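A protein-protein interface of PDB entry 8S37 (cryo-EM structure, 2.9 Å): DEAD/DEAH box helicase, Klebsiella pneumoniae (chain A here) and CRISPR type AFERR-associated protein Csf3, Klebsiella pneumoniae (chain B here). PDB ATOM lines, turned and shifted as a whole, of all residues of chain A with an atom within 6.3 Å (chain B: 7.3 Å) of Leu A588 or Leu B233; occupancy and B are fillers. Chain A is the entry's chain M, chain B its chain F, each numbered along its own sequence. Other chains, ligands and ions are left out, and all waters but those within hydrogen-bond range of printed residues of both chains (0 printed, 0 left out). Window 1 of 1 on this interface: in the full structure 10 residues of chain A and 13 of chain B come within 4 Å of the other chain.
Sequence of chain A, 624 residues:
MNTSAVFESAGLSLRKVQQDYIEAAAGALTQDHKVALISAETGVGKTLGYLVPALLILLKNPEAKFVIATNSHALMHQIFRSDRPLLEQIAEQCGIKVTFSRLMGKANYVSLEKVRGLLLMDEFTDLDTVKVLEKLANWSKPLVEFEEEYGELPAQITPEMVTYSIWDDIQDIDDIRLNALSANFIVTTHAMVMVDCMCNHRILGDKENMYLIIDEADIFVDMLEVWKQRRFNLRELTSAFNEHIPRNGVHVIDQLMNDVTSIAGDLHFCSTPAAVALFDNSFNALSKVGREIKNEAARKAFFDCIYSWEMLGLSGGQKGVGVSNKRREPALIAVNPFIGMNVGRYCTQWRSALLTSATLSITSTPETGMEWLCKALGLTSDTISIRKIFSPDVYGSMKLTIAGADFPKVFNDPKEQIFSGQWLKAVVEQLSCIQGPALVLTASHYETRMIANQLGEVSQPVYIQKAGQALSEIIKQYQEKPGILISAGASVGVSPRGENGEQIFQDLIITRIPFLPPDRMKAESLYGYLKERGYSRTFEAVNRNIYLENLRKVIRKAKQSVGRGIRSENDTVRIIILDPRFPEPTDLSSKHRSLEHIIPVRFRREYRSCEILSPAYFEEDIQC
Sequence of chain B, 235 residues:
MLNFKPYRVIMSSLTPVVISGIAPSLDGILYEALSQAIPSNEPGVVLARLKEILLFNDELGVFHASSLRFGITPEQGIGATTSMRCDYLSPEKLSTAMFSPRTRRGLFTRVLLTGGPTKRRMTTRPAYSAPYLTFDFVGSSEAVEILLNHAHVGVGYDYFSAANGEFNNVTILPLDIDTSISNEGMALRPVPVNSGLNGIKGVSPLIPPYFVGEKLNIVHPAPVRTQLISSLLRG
The side-chain carboxylate (OD1) of Asp A587 lies close to the backbone NH (N) of Ser A589, at 3.3 Å. O of Leu B173 sits at hydrogen-bond distance from N of Arg B8, at 2.9 Å. O of Ile B10 is in hydrogen-bond range of OG1 of Thr B171 (2.8 Å). O of Glu A584 lies within hydrogen-bond range of NH2 of Arg A593 (3.0 Å).
Hydrophobic or aromatic side chains of chain A that line the printed part of chain B: Leu A588. Of the 21 printed residues of chain B, 5 touch a printed residue of chain A. Printed residues of chain B that touch a printed residue of chain A: Tyr B132, Asn B169, Thr B171, Leu B173 and Leu B233. Hydrophobic or aromatic side chains of chain B within 4 Å of the printed part of chain A: Tyr B132, Leu B173 and Leu B233.
ND2 of Asn B169 lies within hydrogen-bond range of O of Leu A588 (3.4 Å). The side-chain hydroxyl (OH) of Tyr B132 sits at hydrogen-bond distance from the backbone NH (N) of Ser A589, 2.6 Å away.
Among the printed residues, pairs that only touch across the chains: Leu A588 with Tyr B132 (2.9 Å), Leu A588 with Leu B233 (3.3 Å), Pro A585 with Leu B233 (3.4 Å), Arg A608 with Leu B173 (3.6 Å), Thr A586 with Leu B233 (3.8 Å), Leu A588 with Thr B171 (3.8 Å) and Arg A593 with Asn B169 (3.9 Å).
Leu A588 touches just these residues of chain B: Tyr B132, Asn B169, Thr B171 and Leu B233. Printed residues of chain A within 4 Å of Leu B233: Pro A585, Thr A586 and Leu A588. Of the printed residues of chain A, Leu B173 touches Arg A608 (3.6 Å). Of the printed residues of chain B, Thr A586 touches Leu B233. Of the printed residues of chain B, Arg A608 touches Leu B173. Of the printed residues of chain B, Ser A589 touches Tyr B132. The nearest residue of chain A that does not touch Leu B233 is Arg A608 (4.4 Å).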
ATOM      1  N   GLU A 584      -2.156  21.838 -22.824  1.00  0.00           N
ATOM      2  CA  GLU A 584      -3.345  21.986 -22.005  1.00  0.00           C
ATOM      3  C   GLU A 584      -3.575  20.720 -21.179  1.00  0.00           C
ATOM      4  O   GLU A 584      -3.144  19.632 -21.570  1.00  0.00           O
ATOM      5  CB  GLU A 584      -4.567  22.268 -22.873  1.00  0.00           C
ATOM      6  CG  GLU A 584      -4.653  23.700 -23.366  1.00  0.00           C
ATOM      7  CD  GLU A 584      -5.937  23.979 -24.123  1.00  0.00           C
ATOM      8  OE1 GLU A 584      -6.706  23.025 -24.362  1.00  0.00           O
ATOM      9  OE2 GLU A 584      -6.177  25.154 -24.475  1.00  0.00           O
ATOM     10  N   PRO A 585      -4.235  20.833 -20.020  1.00  0.00           N
ATOM     11  CA  PRO A 585      -4.543  19.614 -19.254  1.00  0.00           C
ATOM     12  C   PRO A 585      -5.345  18.597 -20.041  1.00  0.00           C
ATOM     13  O   PRO A 585      -5.093  17.392 -19.924  1.00  0.00           O
ATOM     14  CB  PRO A 585      -5.337  20.146 -18.055  1.00  0.00           C
ATOM     15  CG  PRO A 585      -4.931  21.556 -17.921  1.00  0.00           C
ATOM     16  CD  PRO A 585      -4.694  22.042 -19.313  1.00  0.00           C
ATOM     17  N   THR A 586      -6.306  19.048 -20.849  1.00  0.00           N
ATOM     18  CA  THR A 586      -7.147  18.125 -21.598  1.00  0.00           C
ATOM     19  C   THR A 586      -6.443  17.540 -22.813  1.00  0.00           C
ATOM     20  O   THR A 586      -6.858  16.486 -23.304  1.00  0.00           O
ATOM     21  CB  THR A 586      -8.428  18.829 -22.052  1.00  0.00           C
ATOM     22  OG1 THR A 586      -8.098  19.896 -22.951  1.00  0.00           O
ATOM     23  CG2 THR A 586      -9.181  19.393 -20.857  1.00  0.00           C
ATOM     24  N   ASP A 587      -5.396  18.197 -23.309  1.00  0.00           N
ATOM     25  CA  ASP A 587      -4.672  17.744 -24.495  1.00  0.00           C
ATOM     26  C   ASP A 587      -3.530  16.839 -24.052  1.00  0.00           C
ATOM     27  O   ASP A 587      -2.389  17.273 -23.893  1.00  0.00           O
ATOM     28  CB  ASP A 587      -4.176  18.932 -25.308  1.00  0.00           C
ATOM     29  CG  ASP A 587      -3.826  18.556 -26.733  1.00  0.00           C
ATOM     30  OD1 ASP A 587      -3.406  17.402 -26.960  1.00  0.00           O
ATOM     31  OD2 ASP A 587      -3.971  19.416 -27.627  1.00  0.00           O
ATOM     32  N   LEU A 588      -3.834  15.556 -23.866  1.00  0.00           N
ATOM     33  CA  LEU A 588      -2.821  14.582 -23.476  1.00  0.00           C
ATOM     34  C   LEU A 588      -1.989  14.104 -24.656  1.00  0.00           C
ATOM     35  O   LEU A 588      -0.950  13.471 -24.444  1.00  0.00           O
ATOM     36  CB  LEU A 588      -3.476  13.375 -22.800  1.00  0.00           C
ATOM     37  CG  LEU A 588      -3.623  13.427 -21.279  1.00  0.00           C
ATOM     38  CD1 LEU A 588      -2.276  13.233 -20.598  1.00  0.00           C
ATOM     39  CD2 LEU A 588      -4.254  14.735 -20.848  1.00  0.00           C
ATOM     40  N   SER A 589      -2.417  14.400 -25.881  1.00  0.00           N
ATOM     41  CA  SER A 589      -1.701  14.042 -27.095  1.00  0.00           C
ATOM     42  C   SER A 589      -0.955  15.228 -27.685  1.00  0.00           C
ATOM     43  O   SER A 589      -0.514  15.161 -28.837  1.00  0.00           O
ATOM     44  CB  SER A 589      -2.667  13.468 -28.134  1.00  0.00           C
ATOM     45  OG  SER A 589      -3.751  14.352 -28.363  1.00  0.00           O
ATOM     46  N   SER A 590      -0.808  16.312 -26.925  1.00  0.00           N
ATOM     47  CA  SER A 590      -0.168  17.504 -27.454  1.00  0.00           C
ATOM     48  C   SER A 590       1.287  17.213 -27.785  1.00  0.00           C
ATOM     49  O   SER A 590       1.937  16.374 -27.154  1.00  0.00           O
ATOM     50  CB  SER A 590      -0.244  18.648 -26.442  1.00  0.00           C
ATOM     51  OG  SER A 590       0.587  19.726 -26.835  1.00  0.00           O
ATOM     52  N   ARG A 593       4.093  17.404 -25.053  1.00  0.00           N
ATOM     53  CA  ARG A 593       3.528  16.890 -23.810  1.00  0.00           C
ATOM     54  C   ARG A 593       4.585  16.787 -22.718  1.00  0.00           C
ATOM     55  O   ARG A 593       4.269  16.953 -21.536  1.00  0.00           O
ATOM     56  CB  ARG A 593       2.870  15.531 -24.079  1.00  0.00           C
ATOM     57  CG  ARG A 593       2.618  14.607 -22.873  1.00  0.00           C
ATOM     58  CD  ARG A 593       1.751  15.202 -21.760  1.00  0.00           C
ATOM     59  NE  ARG A 593       0.669  16.057 -22.232  1.00  0.00           N
ATOM     60  CZ  ARG A 593      -0.267  16.573 -21.447  1.00  0.00           C
ATOM     61  NH1 ARG A 593      -0.307  16.317 -20.148  1.00  0.00           N
ATOM     62  NH2 ARG A 593      -1.194  17.364 -21.978  1.00  0.00           N
ATOM     63  N   ARG A 608      -3.846  20.316 -13.455  1.00  0.00           N
ATOM     64  CA  ARG A 608      -5.058  19.824 -14.100  1.00  0.00           C
ATOM     65  C   ARG A 608      -6.201  20.821 -13.956  1.00  0.00           C
ATOM     66  O   ARG A 608      -6.932  21.079 -14.919  1.00  0.00           O
ATOM     67  CB  ARG A 608      -5.459  18.472 -13.512  1.00  0.00           C
ATOM     68  CG  ARG A 608      -4.919  17.279 -14.276  1.00  0.00           C
ATOM     69  CD  ARG A 608      -5.306  15.979 -13.600  1.00  0.00           C
ATOM     70  NE  ARG A 608      -4.632  15.821 -12.316  1.00  0.00           N
ATOM     71  CZ  ARG A 608      -3.400  15.351 -12.159  1.00  0.00           C
ATOM     72  NH1 ARG A 608      -2.665  14.967 -13.191  1.00  0.00           N
ATOM     73  NH2 ARG A 608      -2.892  15.265 -10.934  1.00  0.00           N
ATOM     74  N   ARG B   8      -7.252   7.597 -11.173  1.00  0.00           N
ATOM     75  CA  ARG B   8      -7.739   7.360 -12.522  1.00  0.00           C
ATOM     76  C   ARG B   8      -6.536   7.384 -13.450  1.00  0.00           C
ATOM     77  O   ARG B   8      -5.804   8.379 -13.499  1.00  0.00           O
ATOM     78  CB  ARG B   8      -8.764   8.416 -12.933  1.00  0.00           C
ATOM     79  CG  ARG B   8      -9.108   8.415 -14.414  1.00  0.00           C
ATOM     80  CD  ARG B   8     -10.337   9.259 -14.688  1.00  0.00           C
ATOM     81  NE  ARG B   8     -11.548   8.639 -14.162  1.00  0.00           N
ATOM     82  CZ  ARG B   8     -12.735   9.227 -14.114  1.00  0.00           C
ATOM     83  NH1 ARG B   8     -12.915  10.468 -14.537  1.00  0.00           N
ATOM     84  NH2 ARG B   8     -13.771   8.553 -13.625  1.00  0.00           N
ATOM     85  N   ILE B  10      -5.083   7.193 -17.195  1.00  0.00           N
ATOM     86  CA  ILE B  10      -5.391   7.479 -18.590  1.00  0.00           C
ATOM     87  C   ILE B  10      -4.120   7.257 -19.390  1.00  0.00           C
ATOM     88  O   ILE B  10      -3.074   7.835 -19.070  1.00  0.00           O
ATOM     89  CB  ILE B  10      -5.915   8.915 -18.777  1.00  0.00           C
ATOM     90  CG1 ILE B  10      -6.997   9.224 -17.740  1.00  0.00           C
ATOM     91  CG2 ILE B  10      -6.472   9.111 -20.186  1.00  0.00           C
ATOM     92  CD1 ILE B  10      -7.710  10.539 -17.968  1.00  0.00           C
ATOM     93  N   MET B  11      -4.204   6.419 -20.418  1.00  0.00           N
ATOM     94  CA  MET B  11      -3.054   6.064 -21.232  1.00  0.00           C
ATOM     95  C   MET B  11      -3.427   6.178 -22.701  1.00  0.00           C
ATOM     96  O   MET B  11      -4.595   6.052 -23.071  1.00  0.00           O
ATOM     97  CB  MET B  11      -2.581   4.642 -20.924  1.00  0.00           C
ATOM     98  CG  MET B  11      -3.609   3.571 -21.255  1.00  0.00           C
ATOM     99  SD  MET B  11      -3.484   2.114 -20.203  1.00  0.00           S
ATOM    100  CE  MET B  11      -4.122   2.756 -18.660  1.00  0.00           C
ATOM    101  N   SER B  12      -2.427   6.441 -23.535  1.00  0.00           N
ATOM    102  CA  SER B  12      -2.654   6.585 -24.966  1.00  0.00           C
ATOM    103  C   SER B  12      -2.679   5.207 -25.610  1.00  0.00           C
ATOM    104  O   SER B  12      -1.695   4.467 -25.529  1.00  0.00           O
ATOM    105  CB  SER B  12      -1.564   7.450 -25.591  1.00  0.00           C
ATOM    106  OG  SER B  12      -1.434   8.679 -24.902  1.00  0.00           O
ATOM    107  N   THR B  73     -11.418  11.710 -27.655  1.00  0.00           N
ATOM    108  CA  THR B  73     -11.218  13.141 -27.791  1.00  0.00           C
ATOM    109  C   THR B  73     -12.069  13.674 -28.933  1.00  0.00           C
ATOM    110  O   THR B  73     -12.517  12.910 -29.791  1.00  0.00           O
ATOM    111  CB  THR B  73      -9.748  13.439 -28.068  1.00  0.00           C
ATOM    112  OG1 THR B  73      -9.434  13.071 -29.418  1.00  0.00           O
ATOM    113  CG2 THR B  73      -8.861  12.657 -27.121  1.00  0.00           C
ATOM    114  N   TYR B 132      -7.618   7.115 -26.262  1.00  0.00           N
ATOM    115  CA  TYR B 132      -7.195   6.917 -24.882  1.00  0.00           C
ATOM    116  C   TYR B 132      -7.945   5.756 -24.249  1.00  0.00           C
ATOM    117  O   TYR B 132      -9.095   5.481 -24.585  1.00  0.00           O
ATOM    118  CB  TYR B 132      -7.408   8.170 -24.042  1.00  0.00           C
ATOM    119  CG  TYR B 132      -6.536   9.313 -24.471  1.00  0.00           C
ATOM    120  CD1 TYR B 132      -6.942  10.179 -25.468  1.00  0.00           C
ATOM    121  CD2 TYR B 132      -5.302   9.524 -23.882  1.00  0.00           C
ATOM    122  CE1 TYR B 132      -6.147  11.222 -25.869  1.00  0.00           C
ATOM    123  CE2 TYR B 132      -4.499  10.567 -24.275  1.00  0.00           C
ATOM    124  CZ  TYR B 132      -4.928  11.414 -25.269  1.00  0.00           C
ATOM    125  OH  TYR B 132      -4.139  12.461 -25.669  1.00  0.00           O
ATOM    126  N   THR B 134      -8.894   4.356 -20.314  1.00  0.00           N
ATOM    127  CA  THR B 134      -9.015   4.855 -18.956  1.00  0.00           C
ATOM    128  C   THR B 134      -9.478   3.742 -18.033  1.00  0.00           C
ATOM    129  O   THR B 134     -10.341   2.935 -18.397  1.00  0.00           O
ATOM    130  CB  THR B 134      -9.988   6.032 -18.888  1.00  0.00           C
ATOM    131  OG1 THR B 134      -9.439   7.142 -19.605  1.00  0.00           O
ATOM    132  CG2 THR B 134     -10.246   6.441 -17.445  1.00  0.00           C
ATOM    133  N   ASN B 169       2.638   6.528 -22.428  1.00  0.00           N
ATOM    134  CA  ASN B 169       2.282   7.785 -21.780  1.00  0.00           C
ATOM    135  C   ASN B 169       1.178   7.553 -20.748  1.00  0.00           C
ATOM    136  O   ASN B 169       0.100   8.146 -20.792  1.00  0.00           O
ATOM    137  CB  ASN B 169       1.861   8.824 -22.821  1.00  0.00           C
ATOM    138  CG  ASN B 169       1.632  10.194 -22.218  1.00  0.00           C
ATOM    139  OD1 ASN B 169       2.085  10.481 -21.112  1.00  0.00           O
ATOM    140  ND2 ASN B 169       0.923  11.049 -22.946  1.00  0.00           N
ATOM    141  N   VAL B 170       1.470   6.653 -19.813  1.00  0.00           N
ATOM    142  CA  VAL B 170       0.542   6.360 -18.729  1.00  0.00           C
ATOM    143  C   VAL B 170       0.548   7.527 -17.753  1.00  0.00           C
ATOM    144  O   VAL B 170       1.594   7.878 -17.194  1.00  0.00           O
ATOM    145  CB  VAL B 170       0.916   5.048 -18.030  1.00  0.00           C
ATOM    146  CG1 VAL B 170       0.028   4.827 -16.822  1.00  0.00           C
ATOM    147  CG2 VAL B 170       0.803   3.883 -18.999  1.00  0.00           C
ATOM    148  N   THR B 171      -0.617   8.136 -17.545  1.00  0.00           N
ATOM    149  CA  THR B 171      -0.769   9.257 -16.627  1.00  0.00           C
ATOM    150  C   THR B 171      -1.786   8.895 -15.557  1.00  0.00           C
ATOM    151  O   THR B 171      -2.913   8.509 -15.874  1.00  0.00           O
ATOM    152  CB  THR B 171      -1.224  10.514 -17.369  1.00  0.00           C
ATOM    153  OG1 THR B 171      -2.528  10.297 -17.922  1.00  0.00           O
ATOM    154  CG2 THR B 171      -0.255  10.856 -18.488  1.00  0.00           C
ATOM    155  N   LEU B 173      -3.950  10.307 -12.323  1.00  0.00           N
ATOM    156  CA  LEU B 173      -4.473  11.496 -11.679  1.00  0.00           C
ATOM    157  C   LEU B 173      -5.332  11.088 -10.488  1.00  0.00           C
ATOM    158  O   LEU B 173      -6.212  10.231 -10.642  1.00  0.00           O
ATOM    159  CB  LEU B 173      -5.299  12.329 -12.664  1.00  0.00           C
ATOM    160  CG  LEU B 173      -6.559  11.666 -13.217  1.00  0.00           C
ATOM    161  CD1 LEU B 173      -7.801  12.192 -12.512  1.00  0.00           C
ATOM    162  CD2 LEU B 173      -6.655  11.890 -14.710  1.00  0.00           C
ATOM    163  N   LEU B 175      -8.291  10.833  -7.887  1.00  0.00           N
ATOM    164  CA  LEU B 175      -9.713  11.136  -7.906  1.00  0.00           C
ATOM    165  C   LEU B 175     -10.186  11.548  -6.519  1.00  0.00           C
ATOM    166  O   LEU B 175      -9.519  11.308  -5.509  1.00  0.00           O
ATOM    167  CB  LEU B 175     -10.523   9.930  -8.386  1.00  0.00           C
ATOM    168  CG  LEU B 175     -10.355   9.495  -9.840  1.00  0.00           C
ATOM    169  CD1 LEU B 175     -11.159   8.228 -10.076  1.00  0.00           C
ATOM    170  CD2 LEU B 175     -10.781  10.594 -10.802  1.00  0.00           C
ATOM    171  N   GLN B 227     -16.065   7.962 -22.902  1.00  0.00           N
ATOM    172  CA  GLN B 227     -16.190   9.215 -22.180  1.00  0.00           C
ATOM    173  C   GLN B 227     -15.276  10.236 -22.831  1.00  0.00           C
ATOM    174  O   GLN B 227     -14.198   9.890 -23.320  1.00  0.00           O
ATOM    175  CB  GLN B 227     -15.822   9.048 -20.702  1.00  0.00           C
ATOM    176  CG  GLN B 227     -16.318  10.169 -19.809  1.00  0.00           C
ATOM    177  CD  GLN B 227     -17.798  10.059 -19.509  1.00  0.00           C
ATOM    178  OE1 GLN B 227     -18.320   8.966 -19.290  1.00  0.00           O
ATOM    179  NE2 GLN B 227     -18.485  11.195 -19.501  1.00  0.00           N
ATOM    180  N   LEU B 228     -15.714  11.490 -22.852  1.00  0.00           N
ATOM    181  CA  LEU B 228     -14.840  12.556 -23.312  1.00  0.00           C
ATOM    182  C   LEU B 228     -13.613  12.638 -22.415  1.00  0.00           C
ATOM    183  O   LEU B 228     -13.714  12.547 -21.189  1.00  0.00           O
ATOM    184  CB  LEU B 228     -15.583  13.890 -23.320  1.00  0.00           C
ATOM    185  CG  LEU B 228     -16.491  14.128 -24.528  1.00  0.00           C
ATOM    186  CD1 LEU B 228     -17.423  15.299 -24.265  1.00  0.00           C
ATOM    187  CD2 LEU B 228     -15.668  14.372 -25.784  1.00  0.00           C
ATOM    188  N   ILE B 229     -12.444  12.803 -23.036  1.00  0.00           N
ATOM    189  CA  ILE B 229     -11.214  12.900 -22.258  1.00  0.00           C
ATOM    190  C   ILE B 229     -11.264  14.099 -21.326  1.00  0.00           C
ATOM    191  O   ILE B 229     -10.702  14.063 -20.225  1.00  0.00           O
ATOM    192  CB  ILE B 229      -9.985  12.956 -23.186  1.00  0.00           C
ATOM    193  CG1 ILE B 229      -8.710  13.045 -22.351  1.00  0.00           C
ATOM    194  CG2 ILE B 229     -10.058  14.151 -24.136  1.00  0.00           C
ATOM    195  CD1 ILE B 229      -7.504  12.468 -23.028  1.00  0.00           C
ATOM    196  N   SER B 230     -11.926  15.178 -21.744  1.00  0.00           N
ATOM    197  CA  SER B 230     -12.106  16.318 -20.854  1.00  0.00           C
ATOM    198  C   SER B 230     -12.930  15.930 -19.635  1.00  0.00           C
ATOM    199  O   SER B 230     -12.605  16.313 -18.506  1.00  0.00           O
ATOM    200  CB  SER B 230     -12.770  17.469 -21.608  1.00  0.00           C
ATOM    201  OG  SER B 230     -14.029  17.075 -22.122  1.00  0.00           O
ATOM    202  N   SER B 231     -14.002  15.163 -19.845  1.00  0.00           N
ATOM    203  CA  SER B 231     -14.813  14.707 -18.723  1.00  0.00           C
ATOM    204  C   SER B 231     -14.033  13.771 -17.811  1.00  0.00           C
ATOM    205  O   SER B 231     -14.308  13.712 -16.607  1.00  0.00           O
ATOM    206  CB  SER B 231     -16.074  14.014 -19.236  1.00  0.00           C
ATOM    207  OG  SER B 231     -16.883  14.914 -19.972  1.00  0.00           O
ATOM    208  N   LEU B 232     -13.063  13.037 -18.357  1.00  0.00           N
ATOM    209  CA  LEU B 232     -12.298  12.101 -17.542  1.00  0.00           C
ATOM    210  C   LEU B 232     -11.203  12.809 -16.758  1.00  0.00           C
ATOM    211  O   LEU B 232     -10.904  12.427 -15.621  1.00  0.00           O
ATOM    212  CB  LEU B 232     -11.691  11.015 -18.426  1.00  0.00           C
ATOM    213  CG  LEU B 232     -12.683  10.075 -19.109  1.00  0.00           C
ATOM    214  CD1 LEU B 232     -11.978   9.274 -20.187  1.00  0.00           C
ATOM    215  CD2 LEU B 232     -13.337   9.151 -18.094  1.00  0.00           C
ATOM    216  N   LEU B 233     -10.603  13.844 -17.341  1.00  0.00           N
ATOM    217  CA  LEU B 233      -9.589  14.623 -16.645  1.00  0.00           C
ATOM    218  C   LEU B 233     -10.185  15.654 -15.701  1.00  0.00           C
ATOM    219  O   LEU B 233      -9.440  16.268 -14.931  1.00  0.00           O
ATOM    220  CB  LEU B 233      -8.686  15.323 -17.660  1.00  0.00           C
ATOM    221  CG  LEU B 233      -7.694  14.390 -18.354  1.00  0.00           C
ATOM    222  CD1 LEU B 233      -7.381  14.849 -19.766  1.00  0.00           C
ATOM    223  CD2 LEU B 233      -6.418  14.300 -17.533  1.00  0.00           C
ATOM    224  N   ARG B 234     -11.502  15.863 -15.744  1.00  0.00           N
ATOM    225  CA  ARG B 234     -12.129  16.789 -14.810  1.00  0.00           C
ATOM    226  C   ARG B 234     -11.967  16.305 -13.375  1.00  0.00           C
ATOM    227  O   ARG B 234     -11.704  17.103 -12.469  1.00  0.00           O
ATOM    228  CB  ARG B 234     -13.606  16.957 -15.159  1.00  0.00           C
ATOM    229  CG  ARG B 234     -14.232  18.235 -14.613  1.00  0.00           C
ATOM    230  CD  ARG B 234     -15.244  18.834 -15.580  1.00  0.00           C
ATOM    231  NE  ARG B 234     -14.635  19.208 -16.852  1.00  0.00           N
ATOM    232  CZ  ARG B 234     -13.861  20.270 -17.037  1.00  0.00           C
ATOM    233  NH1 ARG B 234     -13.571  21.101 -16.048  1.00  0.00           N
ATOM    234  NH2 ARG B 234     -13.359  20.502 -18.248  1.00  0.00           N
ATOM    235  N   GLY B 235     -12.120  15.004 -13.151  1.00  0.00           N
ATOM    236  CA  GLY B 235     -11.966  14.431 -11.828  1.00  0.00           C
ATOM    237  C   GLY B 235     -13.234  14.511 -11.003  1.00  0.00           C
ATOM    238  O   GLY B 235     -13.382  13.805 -10.004  1.00  0.00           O
